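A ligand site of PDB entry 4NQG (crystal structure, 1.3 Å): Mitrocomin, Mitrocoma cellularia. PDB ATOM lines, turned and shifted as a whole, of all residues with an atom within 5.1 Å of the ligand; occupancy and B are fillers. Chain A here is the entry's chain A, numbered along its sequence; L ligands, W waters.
NE2 of His 176 lies within hydrogen-bond range of OH of Tyr 191 (2.8 Å). A ring nitrogen (NE2) of His 23 is in hydrogen-bond range of the backbone carbonyl oxygen (O) of Trp 180. NE1 of Trp 93 is in hydrogen-bond range of OH of Tyr 89. ND1 of His 176 sits close to O of Met 172 (3.5 Å). The backbone NH of Ile 145 lies within hydrogen-bond range of the backbone carbonyl oxygen of Thr 140, at 3.1 Å. N of Ile 51 is in hydrogen-bond range of O of Lys 46. O of Trp 136 lies within hydrogen-bond range of OG1 of Thr 140 (3.0 Å). O of Ala 143 is in hydrogen-bond range of NZ of Lys 46 (2.6 Å).
Met 26 touches the ligand. CD1 of Leu 30 touches C16 of the ligand, 3.8 Å away. Met 43 touches the ligand. Lys 46 touches the ligand. Ile 51 touches the ligand. CE2 of Phe 73 touches C23 of the ligand (3.7 Å). Ile 112 touches the ligand (O to C12, 3.8 Å). Trp 115 touches the ligand (CH2 to C6, 3.5 Å). Gly 116 touches the ligand (CA to C12, 3.4 Å). CD2 of Leu 119 touches C9 of the ligand (3.7 Å). Phe 120 touches the ligand. Trp 136 touches the ligand (CH2 to O4, 3.8 Å). Ile 145 touches the ligand (CD1 to O5, 3.6 Å). Met 172 touches the ligand (CG to O1, 3.7 Å). Hydrophobic or aromatic side chains that line the ligand: His 23, Met 26, Leu 30, Ile 51, Phe 73, Tyr 89, Trp 93, Ile 112, Trp 115, Leu 119, Phe 120, Trp 136, Tyr 139, Ile 145, Met 172, His 176, Trp 180 and Tyr 191. Within 4 Å of the ligand: His 23, Met 26, Leu 30, Met 43, Lys 46, Ile 51, Phe 73, Tyr 89, Trp 93, Ile 112, Trp 115, Gly 116, Leu 119, Phe 120, Trp 136, Tyr 139, Ile 145, Met 172, His 176, Trp 180 and Tyr 191.
The side-chain hydroxyl (OH) of Tyr 191 lies within hydrogen-bond range of an oxygen (O5) of the ligand (2.7 Å). ND1 of His 23 sits at hydrogen-bond distance from O3 of the ligand, at 2.7 Å. An oxygen (O3) of the ligand is in hydrogen-bond range of the side-chain hydroxyl (OH) of Tyr 89. The side-chain hydroxyl (OH) of Tyr 139 is in hydrogen-bond range of a nitrogen (N1) of the ligand, at 2.8 Å. NE2 of His 176 lies close to O2 of the ligand (3.3 Å). NE1 of Trp 93 sits at hydrogen-bond distance from O3 of the ligand (3.3 Å). An oxygen (O2) of the ligand sits at hydrogen-bond distance from the indole nitrogen of Trp 180, 3.5 Å away.
Water W2 lies within hydrogen-bond range of an oxygen (O1) of the ligand (2.7 Å), the side-chain hydroxyl (OG1) of Thr 173 (2.7 Å) and the backbone carbonyl oxygen (O) of Ile 112 (2.9 Å). Water W1 lies within hydrogen-bond range of OH of Tyr 139 and NE1 of Trp 115.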
ATOM      1  N   HIS A  23      -4.399 -34.644 -18.057  1.00  0.00           N
ATOM      2  CA  HIS A  23      -5.683 -33.932 -18.112  1.00  0.00           C
ATOM      3  C   HIS A  23      -6.659 -34.300 -16.970  1.00  0.00           C
ATOM      4  O   HIS A  23      -7.437 -33.462 -16.573  1.00  0.00           O
ATOM      5  CB  HIS A  23      -6.339 -34.117 -19.489  1.00  0.00           C
ATOM      6  CG  HIS A  23      -5.557 -33.419 -20.533  1.00  0.00           C
ATOM      7  ND1 HIS A  23      -5.450 -32.040 -20.564  1.00  0.00           N
ATOM      8  CD2 HIS A  23      -4.706 -33.892 -21.466  1.00  0.00           C
ATOM      9  CE1 HIS A  23      -4.609 -31.691 -21.513  1.00  0.00           C
ATOM     10  NE2 HIS A  23      -4.155 -32.796 -22.099  1.00  0.00           N
ATOM     11  N   MET A  26      -5.474 -32.084 -14.210  1.00  0.00           N
ATOM     12  CA  MET A  26      -5.969 -30.700 -14.379  1.00  0.00           C
ATOM     13  C   MET A  26      -7.488 -30.581 -14.185  1.00  0.00           C
ATOM     14  O   MET A  26      -7.948 -29.596 -13.640  1.00  0.00           O
ATOM     15  CB  MET A  26      -5.575 -30.110 -15.733  1.00  0.00           C
ATOM     16  CG  MET A  26      -4.064 -29.859 -15.906  1.00  0.00           C
ATOM     17  SD  MET A  26      -3.314 -28.900 -14.584  1.00  0.00           S
ATOM     18  CE  MET A  26      -4.148 -27.360 -14.654  1.00  0.00           C
ATOM     19  N   PHE A  27      -8.255 -31.556 -14.660  1.00  0.00           N
ATOM     20  CA  PHE A  27      -9.702 -31.520 -14.466  1.00  0.00           C
ATOM     21  C   PHE A  27     -10.035 -31.514 -13.008  1.00  0.00           C
ATOM     22  O   PHE A  27     -10.843 -30.680 -12.559  1.00  0.00           O
ATOM     23  CB  PHE A  27     -10.395 -32.724 -15.142  1.00  0.00           C
ATOM     24  CG  PHE A  27     -11.900 -32.692 -15.023  1.00  0.00           C
ATOM     25  CD1 PHE A  27     -12.658 -31.935 -15.917  1.00  0.00           C
ATOM     26  CD2 PHE A  27     -12.557 -33.417 -14.021  1.00  0.00           C
ATOM     27  CE1 PHE A  27     -14.060 -31.923 -15.837  1.00  0.00           C
ATOM     28  CE2 PHE A  27     -13.945 -33.393 -13.924  1.00  0.00           C
ATOM     29  CZ  PHE A  27     -14.697 -32.637 -14.805  1.00  0.00           C
ATOM     30  N   LEU A  30      -9.203 -28.119 -11.521  1.00  0.00           N
ATOM     31  CA  LEU A  30     -10.146 -27.073 -11.930  1.00  0.00           C
ATOM     32  C   LEU A  30     -11.535 -27.244 -11.333  1.00  0.00           C
ATOM     33  O   LEU A  30     -12.281 -26.275 -11.194  1.00  0.00           O
ATOM     34  CB  LEU A  30     -10.259 -27.040 -13.465  1.00  0.00           C
ATOM     35  CG  LEU A  30      -8.950 -26.564 -14.093  1.00  0.00           C
ATOM     36  CD1 LEU A  30      -9.006 -26.737 -15.588  1.00  0.00           C
ATOM     37  CD2 LEU A  30      -8.660 -25.119 -13.711  1.00  0.00           C
ATOM     38  N   MET A  43     -13.361 -20.871 -15.433  1.00  0.00           N
ATOM     39  CA  MET A  43     -12.048 -20.688 -16.004  1.00  0.00           C
ATOM     40  C   MET A  43     -11.705 -19.203 -16.144  1.00  0.00           C
ATOM     41  O   MET A  43     -10.563 -18.779 -15.887  1.00  0.00           O
ATOM     42  CB  MET A  43     -11.922 -21.349 -17.388  1.00  0.00           C
ATOM     43  CG  MET A  43     -12.235 -22.846 -17.440  1.00  0.00           C
ATOM     44  SD  MET A  43     -11.246 -23.897 -16.352  1.00  0.00           S
ATOM     45  CE  MET A  43     -12.293 -23.999 -14.908  1.00  0.00           C
ATOM     46  N   LYS A  46     -11.136 -17.466 -12.778  1.00  0.00           N
ATOM     47  CA  LYS A  46      -9.769 -17.717 -12.363  1.00  0.00           C
ATOM     48  C   LYS A  46      -8.774 -16.825 -13.134  1.00  0.00           C
ATOM     49  O   LYS A  46      -7.859 -16.170 -12.583  1.00  0.00           O
ATOM     50  CB  LYS A  46      -9.463 -19.209 -12.581  1.00  0.00           C
ATOM     51  CG  LYS A  46      -8.113 -19.663 -12.164  1.00  0.00           C
ATOM     52  CD  LYS A  46      -8.057 -21.176 -12.166  1.00  0.00           C
ATOM     53  CE  LYS A  46      -6.658 -21.643 -11.818  1.00  0.00           C
ATOM     54  NZ  LYS A  46      -6.440 -21.423 -10.366  1.00  0.00           N
ATOM     55  N   ALA A  47      -8.898 -16.819 -14.461  1.00  0.00           N
ATOM     56  CA  ALA A  47      -8.018 -16.067 -15.294  1.00  0.00           C
ATOM     57  C   ALA A  47      -8.019 -14.557 -15.037  1.00  0.00           C
ATOM     58  O   ALA A  47      -6.962 -13.925 -14.915  1.00  0.00           O
ATOM     59  CB  ALA A  47      -8.398 -16.353 -16.757  1.00  0.00           C
ATOM     60  N   ILE A  51      -5.874 -14.354 -11.379  1.00  0.00           N
ATOM     61  CA  ILE A  51      -4.534 -14.289 -11.937  1.00  0.00           C
ATOM     62  C   ILE A  51      -4.189 -12.873 -12.466  1.00  0.00           C
ATOM     63  O   ILE A  51      -3.220 -12.269 -12.047  1.00  0.00           O
ATOM     64  CB  ILE A  51      -4.357 -15.386 -13.042  1.00  0.00           C
ATOM     65  CG1 ILE A  51      -4.347 -16.771 -12.380  1.00  0.00           C
ATOM     66  CG2 ILE A  51      -3.126 -15.172 -13.887  1.00  0.00           C
ATOM     67  CD1 ILE A  51      -4.526 -17.945 -13.376  1.00  0.00           C
ATOM     68  N   VAL A  69      -8.108 -17.248 -23.148  1.00  0.00           N
ATOM     69  CA  VAL A  69      -8.606 -18.345 -22.313  1.00  0.00           C
ATOM     70  C   VAL A  69      -9.976 -18.896 -22.791  1.00  0.00           C
ATOM     71  O   VAL A  69     -10.232 -20.137 -22.795  1.00  0.00           O
ATOM     72  CB  VAL A  69      -8.639 -17.868 -20.821  1.00  0.00           C
ATOM     73  CG1 VAL A  69      -9.341 -18.857 -19.894  1.00  0.00           C
ATOM     74  CG2 VAL A  69      -7.188 -17.620 -20.375  1.00  0.00           C
ATOM     75  N   PHE A  72      -9.167 -21.032 -25.855  1.00  0.00           N
ATOM     76  CA  PHE A  72      -8.483 -22.262 -25.511  1.00  0.00           C
ATOM     77  C   PHE A  72      -9.466 -23.278 -24.915  1.00  0.00           C
ATOM     78  O   PHE A  72      -9.634 -24.374 -25.474  1.00  0.00           O
ATOM     79  CB  PHE A  72      -7.327 -21.956 -24.551  1.00  0.00           C
ATOM     80  CG  PHE A  72      -6.577 -23.175 -24.042  1.00  0.00           C
ATOM     81  CD1 PHE A  72      -5.559 -23.748 -24.824  1.00  0.00           C
ATOM     82  CD2 PHE A  72      -6.842 -23.709 -22.786  1.00  0.00           C
ATOM     83  CE1 PHE A  72      -4.839 -24.858 -24.319  1.00  0.00           C
ATOM     84  CE2 PHE A  72      -6.126 -24.780 -22.280  1.00  0.00           C
ATOM     85  CZ  PHE A  72      -5.128 -25.355 -23.038  1.00  0.00           C
ATOM     86  N   PHE A  73     -10.174 -22.906 -23.828  1.00  0.00           N
ATOM     87  CA  PHE A  73     -11.057 -23.873 -23.223  1.00  0.00           C
ATOM     88  C   PHE A  73     -12.279 -24.137 -24.077  1.00  0.00           C
ATOM     89  O   PHE A  73     -12.840 -25.228 -24.045  1.00  0.00           O
ATOM     90  CB  PHE A  73     -11.475 -23.441 -21.812  1.00  0.00           C
ATOM     91  CG  PHE A  73     -10.378 -23.625 -20.809  1.00  0.00           C
ATOM     92  CD1 PHE A  73     -10.062 -24.915 -20.327  1.00  0.00           C
ATOM     93  CD2 PHE A  73      -9.621 -22.559 -20.386  1.00  0.00           C
ATOM     94  CE1 PHE A  73      -9.020 -25.110 -19.462  1.00  0.00           C
ATOM     95  CE2 PHE A  73      -8.582 -22.725 -19.489  1.00  0.00           C
ATOM     96  CZ  PHE A  73      -8.282 -24.016 -19.023  1.00  0.00           C
ATOM     97  N   TYR A  89     -15.182 -33.848 -21.172  1.00  0.00           N
ATOM     98  CA  TYR A  89     -13.983 -33.040 -21.125  1.00  0.00           C
ATOM     99  C   TYR A  89     -12.861 -33.703 -21.907  1.00  0.00           C
ATOM    100  O   TYR A  89     -12.207 -33.054 -22.712  1.00  0.00           O
ATOM    101  CB  TYR A  89     -13.554 -32.830 -19.661  1.00  0.00           C
ATOM    102  CG  TYR A  89     -12.358 -31.915 -19.490  1.00  0.00           C
ATOM    103  CD1 TYR A  89     -12.499 -30.537 -19.657  1.00  0.00           C
ATOM    104  CD2 TYR A  89     -11.112 -32.418 -19.126  1.00  0.00           C
ATOM    105  CE1 TYR A  89     -11.435 -29.675 -19.464  1.00  0.00           C
ATOM    106  CE2 TYR A  89     -10.039 -31.557 -18.898  1.00  0.00           C
ATOM    107  CZ  TYR A  89     -10.213 -30.191 -19.088  1.00  0.00           C
ATOM    108  OH  TYR A  89      -9.186 -29.303 -18.918  1.00  0.00           O
ATOM    109  N   TRP A  93     -10.891 -32.613 -25.263  1.00  0.00           N
ATOM    110  CA  TRP A  93      -9.456 -32.352 -25.292  1.00  0.00           C
ATOM    111  C   TRP A  93      -8.789 -33.120 -26.409  1.00  0.00           C
ATOM    112  O   TRP A  93      -7.771 -32.655 -26.942  1.00  0.00           O
ATOM    113  CB  TRP A  93      -8.820 -32.702 -23.937  1.00  0.00           C
ATOM    114  CG  TRP A  93      -8.448 -31.461 -23.185  1.00  0.00           C
ATOM    115  CD1 TRP A  93      -9.178 -30.816 -22.217  1.00  0.00           C
ATOM    116  CD2 TRP A  93      -7.274 -30.688 -23.406  1.00  0.00           C
ATOM    117  NE1 TRP A  93      -8.487 -29.685 -21.803  1.00  0.00           N
ATOM    118  CE2 TRP A  93      -7.309 -29.602 -22.505  1.00  0.00           C
ATOM    119  CE3 TRP A  93      -6.164 -30.848 -24.244  1.00  0.00           C
ATOM    120  CZ2 TRP A  93      -6.287 -28.650 -22.450  1.00  0.00           C
ATOM    121  CZ3 TRP A  93      -5.140 -29.907 -24.190  1.00  0.00           C
ATOM    122  CH2 TRP A  93      -5.203 -28.833 -23.268  1.00  0.00           C
ATOM    123  N   ILE A 112      -2.735 -22.050 -27.911  1.00  0.00           N
ATOM    124  CA  ILE A 112      -1.849 -22.028 -26.738  1.00  0.00           C
ATOM    125  C   ILE A 112      -0.721 -21.000 -26.895  1.00  0.00           C
ATOM    126  O   ILE A 112      -0.316 -20.366 -25.893  1.00  0.00           O
ATOM    127  CB  ILE A 112      -1.279 -23.470 -26.385  1.00  0.00           C
ATOM    128  CG1 ILE A 112      -0.540 -23.467 -25.043  1.00  0.00           C
ATOM    129  CG2 ILE A 112      -0.342 -23.993 -27.418  1.00  0.00           C
ATOM    130  CD1 ILE A 112      -1.401 -23.252 -23.884  1.00  0.00           C
ATOM    131  N   TRP A 115      -2.333 -17.580 -26.096  1.00  0.00           N
ATOM    132  CA  TRP A 115      -2.441 -17.472 -24.634  1.00  0.00           C
ATOM    133  C   TRP A 115      -1.096 -17.119 -23.986  1.00  0.00           C
ATOM    134  O   TRP A 115      -1.022 -16.211 -23.163  1.00  0.00           O
ATOM    135  CB  TRP A 115      -3.004 -18.779 -24.061  1.00  0.00           C
ATOM    136  CG  TRP A 115      -3.325 -18.751 -22.586  1.00  0.00           C
ATOM    137  CD1 TRP A 115      -3.308 -17.648 -21.740  1.00  0.00           C
ATOM    138  CD2 TRP A 115      -3.686 -19.875 -21.767  1.00  0.00           C
ATOM    139  NE1 TRP A 115      -3.662 -18.031 -20.454  1.00  0.00           N
ATOM    140  CE2 TRP A 115      -3.902 -19.381 -20.448  1.00  0.00           C
ATOM    141  CE3 TRP A 115      -3.892 -21.245 -22.017  1.00  0.00           C
ATOM    142  CZ2 TRP A 115      -4.275 -20.212 -19.379  1.00  0.00           C
ATOM    143  CZ3 TRP A 115      -4.265 -22.086 -20.916  1.00  0.00           C
ATOM    144  CH2 TRP A 115      -4.439 -21.557 -19.633  1.00  0.00           C
ATOM    145  N   GLY A 116      -0.035 -17.830 -24.365  1.00  0.00           N
ATOM    146  CA  GLY A 116       1.270 -17.488 -23.839  1.00  0.00           C
ATOM    147  C   GLY A 116       1.666 -16.034 -24.112  1.00  0.00           C
ATOM    148  O   GLY A 116       2.274 -15.377 -23.257  1.00  0.00           O
ATOM    149  N   LEU A 119      -0.311 -13.842 -21.690  1.00  0.00           N
ATOM    150  CA  LEU A 119       0.127 -13.990 -20.309  1.00  0.00           C
ATOM    151  C   LEU A 119       1.505 -13.350 -20.132  1.00  0.00           C
ATOM    152  O   LEU A 119       1.721 -12.582 -19.169  1.00  0.00           O
ATOM    153  CB  LEU A 119       0.151 -15.467 -19.893  1.00  0.00           C
ATOM    154  CG  LEU A 119       0.649 -15.731 -18.476  1.00  0.00           C
ATOM    155  CD1 LEU A 119      -0.300 -15.068 -17.470  1.00  0.00           C
ATOM    156  CD2 LEU A 119       0.703 -17.231 -18.221  1.00  0.00           C
ATOM    157  N   PHE A 120       2.428 -13.606 -21.046  1.00  0.00           N
ATOM    158  CA  PHE A 120       3.782 -13.068 -20.895  1.00  0.00           C
ATOM    159  C   PHE A 120       3.750 -11.560 -21.012  1.00  0.00           C
ATOM    160  O   PHE A 120       4.578 -10.874 -20.406  1.00  0.00           O
ATOM    161  CB  PHE A 120       4.749 -13.689 -21.902  1.00  0.00           C
ATOM    162  CG  PHE A 120       5.334 -15.012 -21.472  1.00  0.00           C
ATOM    163  CD1 PHE A 120       4.586 -15.968 -20.774  1.00  0.00           C
ATOM    164  CD2 PHE A 120       6.662 -15.287 -21.778  1.00  0.00           C
ATOM    165  CE1 PHE A 120       5.191 -17.187 -20.393  1.00  0.00           C
ATOM    166  CE2 PHE A 120       7.247 -16.497 -21.404  1.00  0.00           C
ATOM    167  CZ  PHE A 120       6.548 -17.428 -20.729  1.00  0.00           C
ATOM    168  N   TRP A 136       8.021 -16.627 -13.190  1.00  0.00           N
ATOM    169  CA  TRP A 136       7.324 -17.895 -13.412  1.00  0.00           C
ATOM    170  C   TRP A 136       6.782 -18.477 -12.090  1.00  0.00           C
ATOM    171  O   TRP A 136       5.660 -18.988 -12.068  1.00  0.00           O
ATOM    172  CB  TRP A 136       8.263 -18.869 -14.121  1.00  0.00           C
ATOM    173  CG  TRP A 136       7.594 -20.161 -14.441  1.00  0.00           C
ATOM    174  CD1 TRP A 136       7.830 -21.372 -13.822  1.00  0.00           C
ATOM    175  CD2 TRP A 136       6.561 -20.394 -15.404  1.00  0.00           C
ATOM    176  NE1 TRP A 136       7.005 -22.340 -14.371  1.00  0.00           N
ATOM    177  CE2 TRP A 136       6.226 -21.765 -15.338  1.00  0.00           C
ATOM    178  CE3 TRP A 136       5.872 -19.560 -16.299  1.00  0.00           C
ATOM    179  CZ2 TRP A 136       5.203 -22.333 -16.138  1.00  0.00           C
ATOM    180  CZ3 TRP A 136       4.886 -20.134 -17.139  1.00  0.00           C
ATOM    181  CH2 TRP A 136       4.549 -21.507 -17.010  1.00  0.00           C
ATOM    182  N   TYR A 139       3.617 -16.456 -11.230  1.00  0.00           N
ATOM    183  CA  TYR A 139       2.450 -16.847 -12.028  1.00  0.00           C
ATOM    184  C   TYR A 139       1.942 -18.216 -11.589  1.00  0.00           C
ATOM    185  O   TYR A 139       0.754 -18.380 -11.270  1.00  0.00           O
ATOM    186  CB  TYR A 139       2.758 -16.895 -13.552  1.00  0.00           C
ATOM    187  CG  TYR A 139       1.643 -17.636 -14.236  1.00  0.00           C
ATOM    188  CD1 TYR A 139       0.367 -17.075 -14.277  1.00  0.00           C
ATOM    189  CD2 TYR A 139       1.820 -18.931 -14.756  1.00  0.00           C
ATOM    190  CE1 TYR A 139      -0.698 -17.746 -14.799  1.00  0.00           C
ATOM    191  CE2 TYR A 139       0.725 -19.645 -15.271  1.00  0.00           C
ATOM    192  CZ  TYR A 139      -0.519 -19.010 -15.327  1.00  0.00           C
ATOM    193  OH  TYR A 139      -1.689 -19.602 -15.787  1.00  0.00           O
ATOM    194  N   THR A 140       2.847 -19.203 -11.606  1.00  0.00           N
ATOM    195  CA  THR A 140       2.349 -20.554 -11.396  1.00  0.00           C
ATOM    196  C   THR A 140       1.780 -20.730  -9.984  1.00  0.00           C
ATOM    197  O   THR A 140       0.816 -21.462  -9.789  1.00  0.00           O
ATOM    198  CB  THR A 140       3.420 -21.629 -11.635  1.00  0.00           C
ATOM    199  OG1 THR A 140       4.537 -21.416 -10.749  1.00  0.00           O
ATOM    200  CG2 THR A 140       3.861 -21.625 -13.096  1.00  0.00           C
ATOM    201  N   ALA A 143      -1.704 -19.077  -9.959  1.00  0.00           N
ATOM    202  CA  ALA A 143      -2.621 -19.979 -10.677  1.00  0.00           C
ATOM    203  C   ALA A 143      -2.848 -21.270  -9.893  1.00  0.00           C
ATOM    204  O   ALA A 143      -3.888 -21.940 -10.022  1.00  0.00           O
ATOM    205  CB  ALA A 143      -2.101 -20.301 -12.075  1.00  0.00           C
ATOM    206  N   ILE A 145      -0.937 -23.970 -10.225  1.00  0.00           N
ATOM    207  CA  ILE A 145      -0.546 -25.126 -11.031  1.00  0.00           C
ATOM    208  C   ILE A 145       0.834 -25.657 -10.619  1.00  0.00           C
ATOM    209  O   ILE A 145       1.124 -26.860 -10.803  1.00  0.00           O
ATOM    210  CB  ILE A 145      -0.604 -24.766 -12.557  1.00  0.00           C
ATOM    211  CG1 ILE A 145      -0.494 -26.027 -13.420  1.00  0.00           C
ATOM    212  CG2 ILE A 145       0.486 -23.766 -12.922  1.00  0.00           C
ATOM    213  CD1 ILE A 145      -0.781 -25.830 -14.955  1.00  0.00           C
ATOM    214  N   VAL A 169       8.703 -17.402 -24.534  1.00  0.00           N
ATOM    215  CA  VAL A 169       7.398 -17.940 -24.902  1.00  0.00           C
ATOM    216  C   VAL A 169       7.488 -18.963 -26.078  1.00  0.00           C
ATOM    217  O   VAL A 169       6.688 -19.883 -26.134  1.00  0.00           O
ATOM    218  CB  VAL A 169       6.419 -16.779 -25.243  1.00  0.00           C
ATOM    219  CG1 VAL A 169       6.836 -16.039 -26.494  1.00  0.00           C
ATOM    220  CG2 VAL A 169       4.998 -17.295 -25.364  1.00  0.00           C
ATOM    221  N   MET A 172       8.447 -22.258 -24.311  1.00  0.00           N
ATOM    222  CA  MET A 172       7.370 -22.826 -23.539  1.00  0.00           C
ATOM    223  C   MET A 172       6.225 -23.303 -24.432  1.00  0.00           C
ATOM    224  O   MET A 172       5.544 -24.283 -24.106  1.00  0.00           O
ATOM    225  CB  MET A 172       6.814 -21.835 -22.485  1.00  0.00           C
ATOM    226  CG  MET A 172       5.954 -22.522 -21.405  1.00  0.00           C
ATOM    227  SD  MET A 172       6.940 -23.806 -20.600  1.00  0.00           S
ATOM    228  CE  MET A 172       6.037 -24.108 -19.095  1.00  0.00           C
ATOM    229  N   THR A 173       5.966 -22.604 -25.529  1.00  0.00           N
ATOM    230  CA  THR A 173       4.967 -23.094 -26.496  1.00  0.00           C
ATOM    231  C   THR A 173       5.371 -24.466 -27.087  1.00  0.00           C
ATOM    232  O   THR A 173       4.506 -25.394 -27.082  1.00  0.00           O
ATOM    233  CB  THR A 173       4.749 -22.097 -27.656  1.00  0.00           C
ATOM    234  OG1 THR A 173       4.322 -20.827 -27.123  1.00  0.00           O
ATOM    235  CG2 THR A 173       3.714 -22.621 -28.660  1.00  0.00           C
ATOM    236  N   HIS A 176       4.761 -27.002 -24.453  1.00  0.00           N
ATOM    237  CA  HIS A 176       3.330 -27.236 -24.271  1.00  0.00           C
ATOM    238  C   HIS A 176       2.734 -28.097 -25.369  1.00  0.00           C
ATOM    239  O   HIS A 176       1.878 -28.921 -25.098  1.00  0.00           O
ATOM    240  CB  HIS A 176       2.593 -25.902 -24.212  1.00  0.00           C
ATOM    241  CG  HIS A 176       2.632 -25.294 -22.855  1.00  0.00           C
ATOM    242  ND1 HIS A 176       2.410 -23.955 -22.627  1.00  0.00           N
ATOM    243  CD2 HIS A 176       2.866 -25.849 -21.640  1.00  0.00           C
ATOM    244  CE1 HIS A 176       2.513 -23.701 -21.333  1.00  0.00           C
ATOM    245  NE2 HIS A 176       2.784 -24.838 -20.708  1.00  0.00           N
ATOM    246  N   TRP A 180       0.892 -31.033 -23.473  1.00  0.00           N
ATOM    247  CA  TRP A 180      -0.568 -31.015 -23.414  1.00  0.00           C
ATOM    248  C   TRP A 180      -1.207 -31.716 -24.603  1.00  0.00           C
ATOM    249  O   TRP A 180      -2.337 -32.231 -24.445  1.00  0.00           O
ATOM    250  CB  TRP A 180      -1.126 -29.593 -23.336  1.00  0.00           C
ATOM    251  CG  TRP A 180      -0.733 -28.786 -22.113  1.00  0.00           C
ATOM    252  CD1 TRP A 180      -0.097 -27.560 -22.088  1.00  0.00           C
ATOM    253  CD2 TRP A 180      -0.939 -29.147 -20.739  1.00  0.00           C
ATOM    254  NE1 TRP A 180       0.082 -27.148 -20.777  1.00  0.00           N
ATOM    255  CE2 TRP A 180      -0.396 -28.113 -19.938  1.00  0.00           C
ATOM    256  CE3 TRP A 180      -1.497 -30.264 -20.110  1.00  0.00           C
ATOM    257  CZ2 TRP A 180      -0.454 -28.149 -18.519  1.00  0.00           C
ATOM    258  CZ3 TRP A 180      -1.539 -30.298 -18.706  1.00  0.00           C
ATOM    259  CH2 TRP A 180      -1.006 -29.244 -17.940  1.00  0.00           C
ATOM    260  N   TYR A 191       6.715 -29.835 -15.794  1.00  0.00           N
ATOM    261  CA  TYR A 191       6.159 -29.108 -14.650  1.00  0.00           C
ATOM    262  C   TYR A 191       6.777 -29.618 -13.354  1.00  0.00           C
ATOM    263  O   TYR A 191       6.267 -29.317 -12.263  1.00  0.00           O
ATOM    264  CB  TYR A 191       4.614 -29.207 -14.651  1.00  0.00           C
ATOM    265  CG  TYR A 191       4.000 -28.154 -15.569  1.00  0.00           C
ATOM    266  CD1 TYR A 191       3.700 -26.891 -15.086  1.00  0.00           C
ATOM    267  CD2 TYR A 191       3.768 -28.399 -16.920  1.00  0.00           C
ATOM    268  CE1 TYR A 191       3.186 -25.902 -15.885  1.00  0.00           C
ATOM    269  CE2 TYR A 191       3.255 -27.370 -17.759  1.00  0.00           C
ATOM    270  CZ  TYR A 191       2.973 -26.126 -17.207  1.00  0.00           C
ATOM    271  OH  TYR A 191       2.469 -25.069 -17.934  1.00  0.00           O
HETATM  272  N1  LIG L   1      -1.498 -22.099 -17.095  1.00  0.00           N
HETATM  273  C1  LIG L   1      -0.371 -22.059 -18.193  1.00  0.00           C
HETATM  274  C2  LIG L   1      -0.811 -23.305 -18.991  1.00  0.00           C
HETATM  275  N2  LIG L   1      -1.894 -23.768 -18.428  1.00  0.00           N
HETATM  276  C3  LIG L   1      -2.626 -24.941 -18.892  1.00  0.00           C
HETATM  277  C4  LIG L   1      -3.749 -25.330 -18.210  1.00  0.00           C
HETATM  278  N3  LIG L   1      -4.164 -24.620 -17.037  1.00  0.00           N
HETATM  279  C5  LIG L   1      -3.495 -23.562 -16.636  1.00  0.00           C
HETATM  280  C6  LIG L   1      -2.300 -23.144 -17.374  1.00  0.00           C
HETATM  281  C7  LIG L   1      -0.484 -20.732 -18.939  1.00  0.00           C
HETATM  282  C8  LIG L   1       0.557 -20.601 -19.999  1.00  0.00           C
HETATM  283  C9  LIG L   1       1.883 -20.402 -19.666  1.00  0.00           C
HETATM  284  C10 LIG L   1       2.848 -20.311 -20.660  1.00  0.00           C
HETATM  285  C11 LIG L   1       2.467 -20.410 -21.993  1.00  0.00           C
HETATM  286  C12 LIG L   1       1.132 -20.599 -22.360  1.00  0.00           C
HETATM  287  C13 LIG L   1       0.171 -20.711 -21.345  1.00  0.00           C
HETATM  288  O1  LIG L   1       3.426 -20.319 -22.968  1.00  0.00           O
HETATM  289  O2  LIG L   1      -0.236 -23.754 -19.993  1.00  0.00           O
HETATM  290  C14 LIG L   1      -4.483 -26.587 -18.563  1.00  0.00           C
HETATM  291  C15 LIG L   1      -5.743 -26.765 -17.994  1.00  0.00           C
HETATM  292  C16 LIG L   1      -6.484 -27.925 -18.236  1.00  0.00           C
HETATM  293  C17 LIG L   1      -5.924 -28.946 -18.981  1.00  0.00           C
HETATM  294  C18 LIG L   1      -4.636 -28.816 -19.500  1.00  0.00           C
HETATM  295  C19 LIG L   1      -3.911 -27.636 -19.306  1.00  0.00           C
HETATM  296  O3  LIG L   1      -6.633 -30.115 -19.137  1.00  0.00           O
HETATM  297  C20 LIG L   1      -3.879 -22.769 -15.423  1.00  0.00           C
HETATM  298  C21 LIG L   1      -5.113 -21.997 -15.681  1.00  0.00           C
HETATM  299  C22 LIG L   1      -6.317 -22.673 -15.774  1.00  0.00           C
HETATM  300  C23 LIG L   1      -7.470 -21.954 -16.005  1.00  0.00           C
HETATM  301  C24 LIG L   1      -7.437 -20.571 -16.096  1.00  0.00           C
HETATM  302  C25 LIG L   1      -6.228 -19.894 -15.990  1.00  0.00           C
HETATM  303  C26 LIG L   1      -5.067 -20.612 -15.777  1.00  0.00           C
HETATM  304  O4  LIG L   1       0.894 -22.275 -17.632  1.00  0.00           O
HETATM  305  O5  LIG L   1       0.950 -23.229 -16.764  1.00  0.00           O
HETATM  306  O   HOH W   1      -3.445 -17.797 -17.004  1.00  0.00           O
HETATM  307  O   HOH W   2       2.395 -21.298 -25.249  1.00  0.00           O
